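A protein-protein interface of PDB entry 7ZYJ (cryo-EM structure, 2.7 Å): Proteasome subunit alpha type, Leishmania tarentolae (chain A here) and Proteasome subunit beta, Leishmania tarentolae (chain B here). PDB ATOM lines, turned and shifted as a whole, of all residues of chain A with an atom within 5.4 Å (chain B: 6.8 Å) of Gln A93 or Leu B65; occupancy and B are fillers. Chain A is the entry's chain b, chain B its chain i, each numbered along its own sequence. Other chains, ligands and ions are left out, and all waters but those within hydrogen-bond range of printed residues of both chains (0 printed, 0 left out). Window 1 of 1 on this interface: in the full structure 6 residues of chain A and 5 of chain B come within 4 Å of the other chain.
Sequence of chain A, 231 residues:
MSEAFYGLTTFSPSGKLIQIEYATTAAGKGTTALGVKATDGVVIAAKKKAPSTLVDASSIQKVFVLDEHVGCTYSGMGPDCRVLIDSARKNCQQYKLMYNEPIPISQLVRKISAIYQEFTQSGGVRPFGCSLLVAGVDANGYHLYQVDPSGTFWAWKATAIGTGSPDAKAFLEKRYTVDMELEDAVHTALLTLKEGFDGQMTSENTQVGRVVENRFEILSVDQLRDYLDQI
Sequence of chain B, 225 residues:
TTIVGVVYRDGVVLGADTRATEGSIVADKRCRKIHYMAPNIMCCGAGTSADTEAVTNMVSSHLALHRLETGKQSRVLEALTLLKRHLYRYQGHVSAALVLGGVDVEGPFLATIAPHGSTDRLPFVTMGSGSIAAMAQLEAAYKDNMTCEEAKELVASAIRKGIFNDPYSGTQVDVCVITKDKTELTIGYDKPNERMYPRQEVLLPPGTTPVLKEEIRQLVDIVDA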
ATOM      1  N   ASP A  67      16.672   5.456  11.465  1.00  0.00           N
ATOM      2  CA  ASP A  67      16.265   6.309  12.569  1.00  0.00           C
ATOM      3  C   ASP A  67      16.723   5.646  13.861  1.00  0.00           C
ATOM      4  O   ASP A  67      17.354   4.586  13.846  1.00  0.00           O
ATOM      5  CB  ASP A  67      14.754   6.554  12.565  1.00  0.00           C
ATOM      6  CG  ASP A  67      14.389   7.946  13.040  1.00  0.00           C
ATOM      7  OD1 ASP A  67      15.217   8.573  13.731  1.00  0.00           O
ATOM      8  OD2 ASP A  67      13.275   8.411  12.725  1.00  0.00           O
ATOM      9  N   ASP A  86      18.687   7.475   1.906  1.00  0.00           N
ATOM     10  CA  ASP A  86      18.435   8.880   2.204  1.00  0.00           C
ATOM     11  C   ASP A  86      16.945   9.195   2.212  1.00  0.00           C
ATOM     12  O   ASP A  86      16.471   9.930   3.088  1.00  0.00           O
ATOM     13  CB  ASP A  86      19.162   9.768   1.195  1.00  0.00           C
ATOM     14  CG  ASP A  86      20.667   9.603   1.257  1.00  0.00           C
ATOM     15  OD1 ASP A  86      21.157   8.969   2.214  1.00  0.00           O
ATOM     16  OD2 ASP A  86      21.361  10.106   0.348  1.00  0.00           O
ATOM     17  N   ALA A  88      14.509   7.111   2.908  1.00  0.00           N
ATOM     18  CA  ALA A  88      13.936   6.508   4.106  1.00  0.00           C
ATOM     19  C   ALA A  88      14.254   7.330   5.348  1.00  0.00           C
ATOM     20  O   ALA A  88      13.394   7.509   6.217  1.00  0.00           O
ATOM     21  CB  ALA A  88      14.442   5.076   4.265  1.00  0.00           C
ATOM     22  N   ARG A  89      15.488   7.831   5.454  1.00  0.00           N
ATOM     23  CA  ARG A  89      15.837   8.681   6.589  1.00  0.00           C
ATOM     24  C   ARG A  89      14.998   9.954   6.599  1.00  0.00           C
ATOM     25  O   ARG A  89      14.497  10.375   7.653  1.00  0.00           O
ATOM     26  CB  ARG A  89      17.328   9.015   6.550  1.00  0.00           C
ATOM     27  CG  ARG A  89      18.231   7.847   6.904  1.00  0.00           C
ATOM     28  CD  ARG A  89      19.663   8.101   6.471  1.00  0.00           C
ATOM     29  NE  ARG A  89      20.599   7.223   7.160  1.00  0.00           N
ATOM     30  CZ  ARG A  89      21.884   7.107   6.855  1.00  0.00           C
ATOM     31  NH1 ARG A  89      22.425   7.801   5.868  1.00  0.00           N
ATOM     32  NH2 ARG A  89      22.644   6.271   7.556  1.00  0.00           N
ATOM     33  N   LYS A  90      14.822  10.573   5.430  1.00  0.00           N
ATOM     34  CA  LYS A  90      14.006  11.778   5.347  1.00  0.00           C
ATOM     35  C   LYS A  90      12.552  11.487   5.700  1.00  0.00           C
ATOM     36  O   LYS A  90      11.892  12.295   6.363  1.00  0.00           O
ATOM     37  CB  LYS A  90      14.116  12.387   3.951  1.00  0.00           C
ATOM     38  CG  LYS A  90      13.418  13.724   3.799  1.00  0.00           C
ATOM     39  CD  LYS A  90      13.579  14.266   2.391  1.00  0.00           C
ATOM     40  CE  LYS A  90      15.007  14.717   2.136  1.00  0.00           C
ATOM     41  NZ  LYS A  90      15.373  15.903   2.959  1.00  0.00           N
ATOM     42  N   ASN A  91      12.034  10.337   5.262  1.00  0.00           N
ATOM     43  CA  ASN A  91      10.664   9.958   5.596  1.00  0.00           C
ATOM     44  C   ASN A  91      10.503   9.749   7.096  1.00  0.00           C
ATOM     45  O   ASN A  91       9.496  10.157   7.686  1.00  0.00           O
ATOM     46  CB  ASN A  91      10.266   8.696   4.832  1.00  0.00           C
ATOM     47  CG  ASN A  91       9.862   8.983   3.404  1.00  0.00           C
ATOM     48  OD1 ASN A  91       9.344  10.056   3.097  1.00  0.00           O
ATOM     49  ND2 ASN A  91      10.096   8.024   2.519  1.00  0.00           N
ATOM     50  N   CYS A  92      11.485   9.102   7.728  1.00  0.00           N
ATOM     51  CA  CYS A  92      11.434   8.913   9.174  1.00  0.00           C
ATOM     52  C   CYS A  92      11.432  10.253   9.901  1.00  0.00           C
ATOM     53  O   CYS A  92      10.661  10.458  10.849  1.00  0.00           O
ATOM     54  CB  CYS A  92      12.617   8.061   9.634  1.00  0.00           C
ATOM     55  SG  CYS A  92      12.574   6.337   9.105  1.00  0.00           S
ATOM     56  N   GLN A  93      12.288  11.181   9.464  1.00  0.00           N
ATOM     57  CA  GLN A  93      12.324  12.496  10.096  1.00  0.00           C
ATOM     58  C   GLN A  93      11.010  13.243   9.903  1.00  0.00           C
ATOM     59  O   GLN A  93      10.512  13.887  10.835  1.00  0.00           O
ATOM     60  CB  GLN A  93      13.495  13.312   9.546  1.00  0.00           C
ATOM     61  CG  GLN A  93      14.849  12.904  10.101  1.00  0.00           C
ATOM     62  CD  GLN A  93      14.898  12.921  11.615  1.00  0.00           C
ATOM     63  OE1 GLN A  93      14.283  13.769  12.260  1.00  0.00           O
ATOM     64  NE2 GLN A  93      15.635  11.981  12.192  1.00  0.00           N
ATOM     65  N   GLN A  94      10.429  13.165   8.704  1.00  0.00           N
ATOM     66  CA  GLN A  94       9.157  13.833   8.452  1.00  0.00           C
ATOM     67  C   GLN A  94       8.044  13.241   9.306  1.00  0.00           C
ATOM     68  O   GLN A  94       7.187  13.972   9.817  1.00  0.00           O
ATOM     69  CB  GLN A  94       8.803  13.742   6.969  1.00  0.00           C
ATOM     70  CG  GLN A  94       9.321  14.900   6.139  1.00  0.00           C
ATOM     71  CD  GLN A  94       9.557  14.519   4.691  1.00  0.00           C
ATOM     72  OE1 GLN A  94       9.046  13.507   4.213  1.00  0.00           O
ATOM     73  NE2 GLN A  94      10.335  15.330   3.985  1.00  0.00           N
ATOM     74  N   TYR A  95       8.035  11.916   9.467  1.00  0.00           N
ATOM     75  CA  TYR A  95       7.033  11.283  10.316  1.00  0.00           C
ATOM     76  C   TYR A  95       7.183  11.729  11.764  1.00  0.00           C
ATOM     77  O   TYR A  95       6.191  12.029  12.438  1.00  0.00           O
ATOM     78  CB  TYR A  95       7.136   9.762  10.209  1.00  0.00           C
ATOM     79  CG  TYR A  95       5.966   9.029  10.825  1.00  0.00           C
ATOM     80  CD1 TYR A  95       5.893   8.822  12.196  1.00  0.00           C
ATOM     81  CD2 TYR A  95       4.935   8.544  10.035  1.00  0.00           C
ATOM     82  CE1 TYR A  95       4.829   8.154  12.761  1.00  0.00           C
ATOM     83  CE2 TYR A  95       3.868   7.875  10.591  1.00  0.00           C
ATOM     84  CZ  TYR A  95       3.819   7.683  11.955  1.00  0.00           C
ATOM     85  OH  TYR A  95       2.755   7.015  12.515  1.00  0.00           O
ATOM     86  N   LYS A  96       8.420  11.770  12.267  1.00  0.00           N
ATOM     87  CA  LYS A  96       8.628  12.246  13.631  1.00  0.00           C
ATOM     88  C   LYS A  96       8.210  13.703  13.784  1.00  0.00           C
ATOM     89  O   LYS A  96       7.713  14.098  14.844  1.00  0.00           O
ATOM     90  CB  LYS A  96      10.086  12.065  14.048  1.00  0.00           C
ATOM     91  CG  LYS A  96      10.404  10.681  14.581  1.00  0.00           C
ATOM     92  CD  LYS A  96      11.833  10.593  15.081  1.00  0.00           C
ATOM     93  CE  LYS A  96      12.133   9.214  15.643  1.00  0.00           C
ATOM     94  NZ  LYS A  96      13.544   9.094  16.099  1.00  0.00           N
ATOM     95  N   LEU A  97       8.409  14.514  12.744  1.00  0.00           N
ATOM     96  CA  LEU A  97       7.960  15.901  12.798  1.00  0.00           C
ATOM     97  C   LEU A  97       6.439  15.992  12.811  1.00  0.00           C
ATOM     98  O   LEU A  97       5.867  16.873  13.464  1.00  0.00           O
ATOM     99  CB  LEU A  97       8.532  16.682  11.616  1.00  0.00           C
ATOM    100  CG  LEU A  97       9.929  17.278  11.789  1.00  0.00           C
ATOM    101  CD1 LEU A  97      10.292  18.132  10.588  1.00  0.00           C
ATOM    102  CD2 LEU A  97      10.017  18.086  13.072  1.00  0.00           C
ATOM    103  N   MET A  98       5.765  15.090  12.094  1.00  0.00           N
ATOM    104  CA  MET A  98       4.318  15.196  11.934  1.00  0.00           C
ATOM    105  C   MET A  98       3.559  14.660  13.144  1.00  0.00           C
ATOM    106  O   MET A  98       2.602  15.291  13.603  1.00  0.00           O
ATOM    107  CB  MET A  98       3.878  14.459  10.669  1.00  0.00           C
ATOM    108  CG  MET A  98       2.379  14.500  10.410  1.00  0.00           C
ATOM    109  SD  MET A  98       1.764  16.150  10.030  1.00  0.00           S
ATOM    110  CE  MET A  98       2.368  16.360   8.358  1.00  0.00           C
ATOM    111  N   ASN B  57      12.159  22.249  16.653  1.00  0.00           N
ATOM    112  CA  ASN B  57      11.918  20.888  16.189  1.00  0.00           C
ATOM    113  C   ASN B  57      12.478  20.674  14.791  1.00  0.00           C
ATOM    114  O   ASN B  57      13.114  19.648  14.520  1.00  0.00           O
ATOM    115  CB  ASN B  57      10.421  20.581  16.217  1.00  0.00           C
ATOM    116  CG  ASN B  57       9.920  20.250  17.604  1.00  0.00           C
ATOM    117  OD1 ASN B  57      10.678  19.790  18.457  1.00  0.00           O
ATOM    118  ND2 ASN B  57       8.635  20.485  17.841  1.00  0.00           N
ATOM    119  N   SER B  60      16.312  20.633  14.903  1.00  0.00           N
ATOM    120  CA  SER B  60      16.784  19.411  15.545  1.00  0.00           C
ATOM    121  C   SER B  60      16.644  18.207  14.620  1.00  0.00           C
ATOM    122  O   SER B  60      17.545  17.362  14.551  1.00  0.00           O
ATOM    123  CB  SER B  60      16.025  19.181  16.850  1.00  0.00           C
ATOM    124  OG  SER B  60      16.303  17.899  17.384  1.00  0.00           O
ATOM    125  N   SER B  61      15.523  18.110  13.900  1.00  0.00           N
ATOM    126  CA  SER B  61      15.350  17.019  12.946  1.00  0.00           C
ATOM    127  C   SER B  61      16.378  17.099  11.823  1.00  0.00           C
ATOM    128  O   SER B  61      16.955  16.079  11.416  1.00  0.00           O
ATOM    129  CB  SER B  61      13.931  17.044  12.378  1.00  0.00           C
ATOM    130  OG  SER B  61      13.772  16.079  11.355  1.00  0.00           O
ATOM    131  N   HIS B  62      16.620  18.307  11.310  1.00  0.00           N
ATOM    132  CA  HIS B  62      17.612  18.478  10.256  1.00  0.00           C
ATOM    133  C   HIS B  62      19.006  18.113  10.755  1.00  0.00           C
ATOM    134  O   HIS B  62      19.791  17.494  10.030  1.00  0.00           O
ATOM    135  CB  HIS B  62      17.577  19.914   9.738  1.00  0.00           C
ATOM    136  CG  HIS B  62      18.450  20.149   8.546  1.00  0.00           C
ATOM    137  ND1 HIS B  62      17.986  20.055   7.251  1.00  0.00           N
ATOM    138  CD2 HIS B  62      19.764  20.464   8.451  1.00  0.00           C
ATOM    139  CE1 HIS B  62      18.974  20.309   6.412  1.00  0.00           C
ATOM    140  NE2 HIS B  62      20.063  20.559   7.114  1.00  0.00           N
ATOM    141  N   LEU B  63      19.327  18.482  11.998  1.00  0.00           N
ATOM    142  CA  LEU B  63      20.613  18.107  12.576  1.00  0.00           C
ATOM    143  C   LEU B  63      20.733  16.599  12.733  1.00  0.00           C
ATOM    144  O   LEU B  63      21.803  16.033  12.499  1.00  0.00           O
ATOM    145  CB  LEU B  63      20.810  18.793  13.926  1.00  0.00           C
ATOM    146  CG  LEU B  63      21.170  20.276  13.937  1.00  0.00           C
ATOM    147  CD1 LEU B  63      21.497  20.702  15.354  1.00  0.00           C
ATOM    148  CD2 LEU B  63      22.333  20.564  13.004  1.00  0.00           C
ATOM    149  N   ALA B  64      19.657  15.933  13.158  1.00  0.00           N
ATOM    150  CA  ALA B  64      19.699  14.479  13.278  1.00  0.00           C
ATOM    151  C   ALA B  64      19.955  13.828  11.926  1.00  0.00           C
ATOM    152  O   ALA B  64      20.770  12.901  11.811  1.00  0.00           O
ATOM    153  CB  ALA B  64      18.397  13.963  13.888  1.00  0.00           C
ATOM    154  N   LEU B  65      19.281  14.317  10.883  1.00  0.00           N
ATOM    155  CA  LEU B  65      19.538  13.819   9.535  1.00  0.00           C
ATOM    156  C   LEU B  65      20.986  14.070   9.128  1.00  0.00           C
ATOM    157  O   LEU B  65      21.634  13.213   8.512  1.00  0.00           O
ATOM    158  CB  LEU B  65      18.577  14.480   8.546  1.00  0.00           C
ATOM    159  CG  LEU B  65      18.309  13.725   7.245  1.00  0.00           C
ATOM    160  CD1 LEU B  65      17.423  12.523   7.509  1.00  0.00           C
ATOM    161  CD2 LEU B  65      17.678  14.641   6.212  1.00  0.00           C
ATOM    162  N   HIS B  66      21.511  15.247   9.470  1.00  0.00           N
ATOM    163  CA  HIS B  66      22.884  15.580   9.110  1.00  0.00           C
ATOM    164  C   HIS B  66      23.892  14.683   9.818  1.00  0.00           C
ATOM    165  O   HIS B  66      24.891  14.287   9.215  1.00  0.00           O
ATOM    166  CB  HIS B  66      23.163  17.048   9.420  1.00  0.00           C
ATOM    167  CG  HIS B  66      24.505  17.515   8.956  1.00  0.00           C
ATOM    168  ND1 HIS B  66      25.514  17.863   9.828  1.00  0.00           N
ATOM    169  CD2 HIS B  66      25.005  17.691   7.711  1.00  0.00           C
ATOM    170  CE1 HIS B  66      26.579  18.231   9.139  1.00  0.00           C
ATOM    171  NE2 HIS B  66      26.296  18.137   7.852  1.00  0.00           N
ATOM    172  N   ARG B  67      23.656  14.353  11.091  1.00  0.00           N
ATOM    173  CA  ARG B  67      24.564  13.437  11.779  1.00  0.00           C
ATOM    174  C   ARG B  67      24.418  12.012  11.271  1.00  0.00           C
ATOM    175  O   ARG B  67      25.380  11.239  11.328  1.00  0.00           O
ATOM    176  CB  ARG B  67      24.343  13.462  13.293  1.00  0.00           C
ATOM    177  CG  ARG B  67      24.118  14.823  13.895  1.00  0.00           C
ATOM    178  CD  ARG B  67      24.226  14.761  15.403  1.00  0.00           C
ATOM    179  NE  ARG B  67      23.362  13.725  15.954  1.00  0.00           N
ATOM    180  CZ  ARG B  67      22.169  13.952  16.486  1.00  0.00           C
ATOM    181  NH1 ARG B  67      21.667  15.172  16.561  1.00  0.00           N
ATOM    182  NH2 ARG B  67      21.461  12.927  16.951  1.00  0.00           N
ATOM    183  N   LEU B  68      23.234  11.640  10.785  1.00  0.00           N
ATOM    184  CA  LEU B  68      23.117  10.358  10.100  1.00  0.00           C
ATOM    185  C   LEU B  68      23.952  10.349   8.825  1.00  0.00           C
ATOM    186  O   LEU B  68      24.591   9.342   8.498  1.00  0.00           O
ATOM    187  CB  LEU B  68      21.654  10.054   9.787  1.00  0.00           C
ATOM    188  CG  LEU B  68      20.872   9.339  10.888  1.00  0.00           C
ATOM    189  CD1 LEU B  68      19.471   9.008  10.412  1.00  0.00           C
ATOM    190  CD2 LEU B  68      21.603   8.083  11.332  1.00  0.00           C
ATOM    191  N   GLU B  69      23.957  11.465   8.097  1.00  0.00           N
ATOM    192  CA  GLU B  69      24.732  11.553   6.863  1.00  0.00           C
ATOM    193  C   GLU B  69      26.234  11.531   7.141  1.00  0.00           C
ATOM    194  O   GLU B  69      26.981  10.764   6.523  1.00  0.00           O
ATOM    195  CB  GLU B  69      24.345  12.818   6.094  1.00  0.00           C
ATOM    196  CG  GLU B  69      25.190  13.077   4.861  1.00  0.00           C
ATOM    197  CD  GLU B  69      24.746  14.308   4.099  1.00  0.00           C
ATOM    198  OE1 GLU B  69      25.133  15.426   4.499  1.00  0.00           O
ATOM    199  OE2 GLU B  69      24.009  14.160   3.102  1.00  0.00           O
ATOM    200  N   THR B  70      26.697  12.371   8.070  1.00  0.00           N
ATOM    201  CA  THR B  70      28.133  12.533   8.283  1.00  0.00           C
ATOM    202  C   THR B  70      28.702  11.472   9.217  1.00  0.00           C
ATOM    203  O   THR B  70      29.830  11.010   9.016  1.00  0.00           O
ATOM    204  CB  THR B  70      28.438  13.925   8.842  1.00  0.00           C
ATOM    205  OG1 THR B  70      28.080  13.977  10.228  1.00  0.00           O
ATOM    206  CG2 THR B  70      27.669  14.995   8.087  1.00  0.00           C
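OG of Ser B61 sits at hydrogen-bond distance from OE1 of Gln A93, at 2.5 Å.
Among the printed residues, pairs that only touch across the chains: Arg A89 with Leu B65 (3.6 Å), Gln A93 with Leu B65 (3.7 Å), Arg A89 with Leu B68 (3.7 Å), Leu A97 with Asn B57 (3.8 Å), Gln A93 with Ala B64 (3.8 Å) and Lys A90 with Leu B65 (3.9 Å).
Leu B65 touches just these residues of chain A: Arg A89 (3.6 Å), Lys A90 (3.9 Å) and Gln A93 (3.7 Å).
Printed residues of chain B within 4 Å of Arg A89: Leu B65 (3.6 Å) and Leu B68 (3.7 Å).
Of the printed residues of chain B, Lys A90 touches Leu B65.
Printed residues of chain B within 4 Å of Leu A97: Asn B57 (3.8 Å).
Tyr A95 touches none of the printed residues of chain B.
His B66 touches none of the printed residues of chain A.
The nearest printed residue of chain B that does not touch Gln A93 is Leu B68 (5.2 Å).
The nearest printed residue of chain B that does not touch Arg A89 is Glu B69 (4.5 Å).
Of the 12 printed residues of chain B, 5 touch a printed residue of chain A.
Printed residues of chain B that touch a printed residue of chain A: Asn B57, Ser B61, Ala B64, Leu B65 and Leu B68.
Of the 13 printed residues of chain A, 4 touch a printed residue of chain B.
Hydrophobic or aromatic side chains of chain A within 4 Å of the printed part of chain B: Leu A97.
Among the printed residues, no Asp or Glu carboxylate lies within 4 Å of a Lys or Arg side-chain nitrogen of the other chain.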
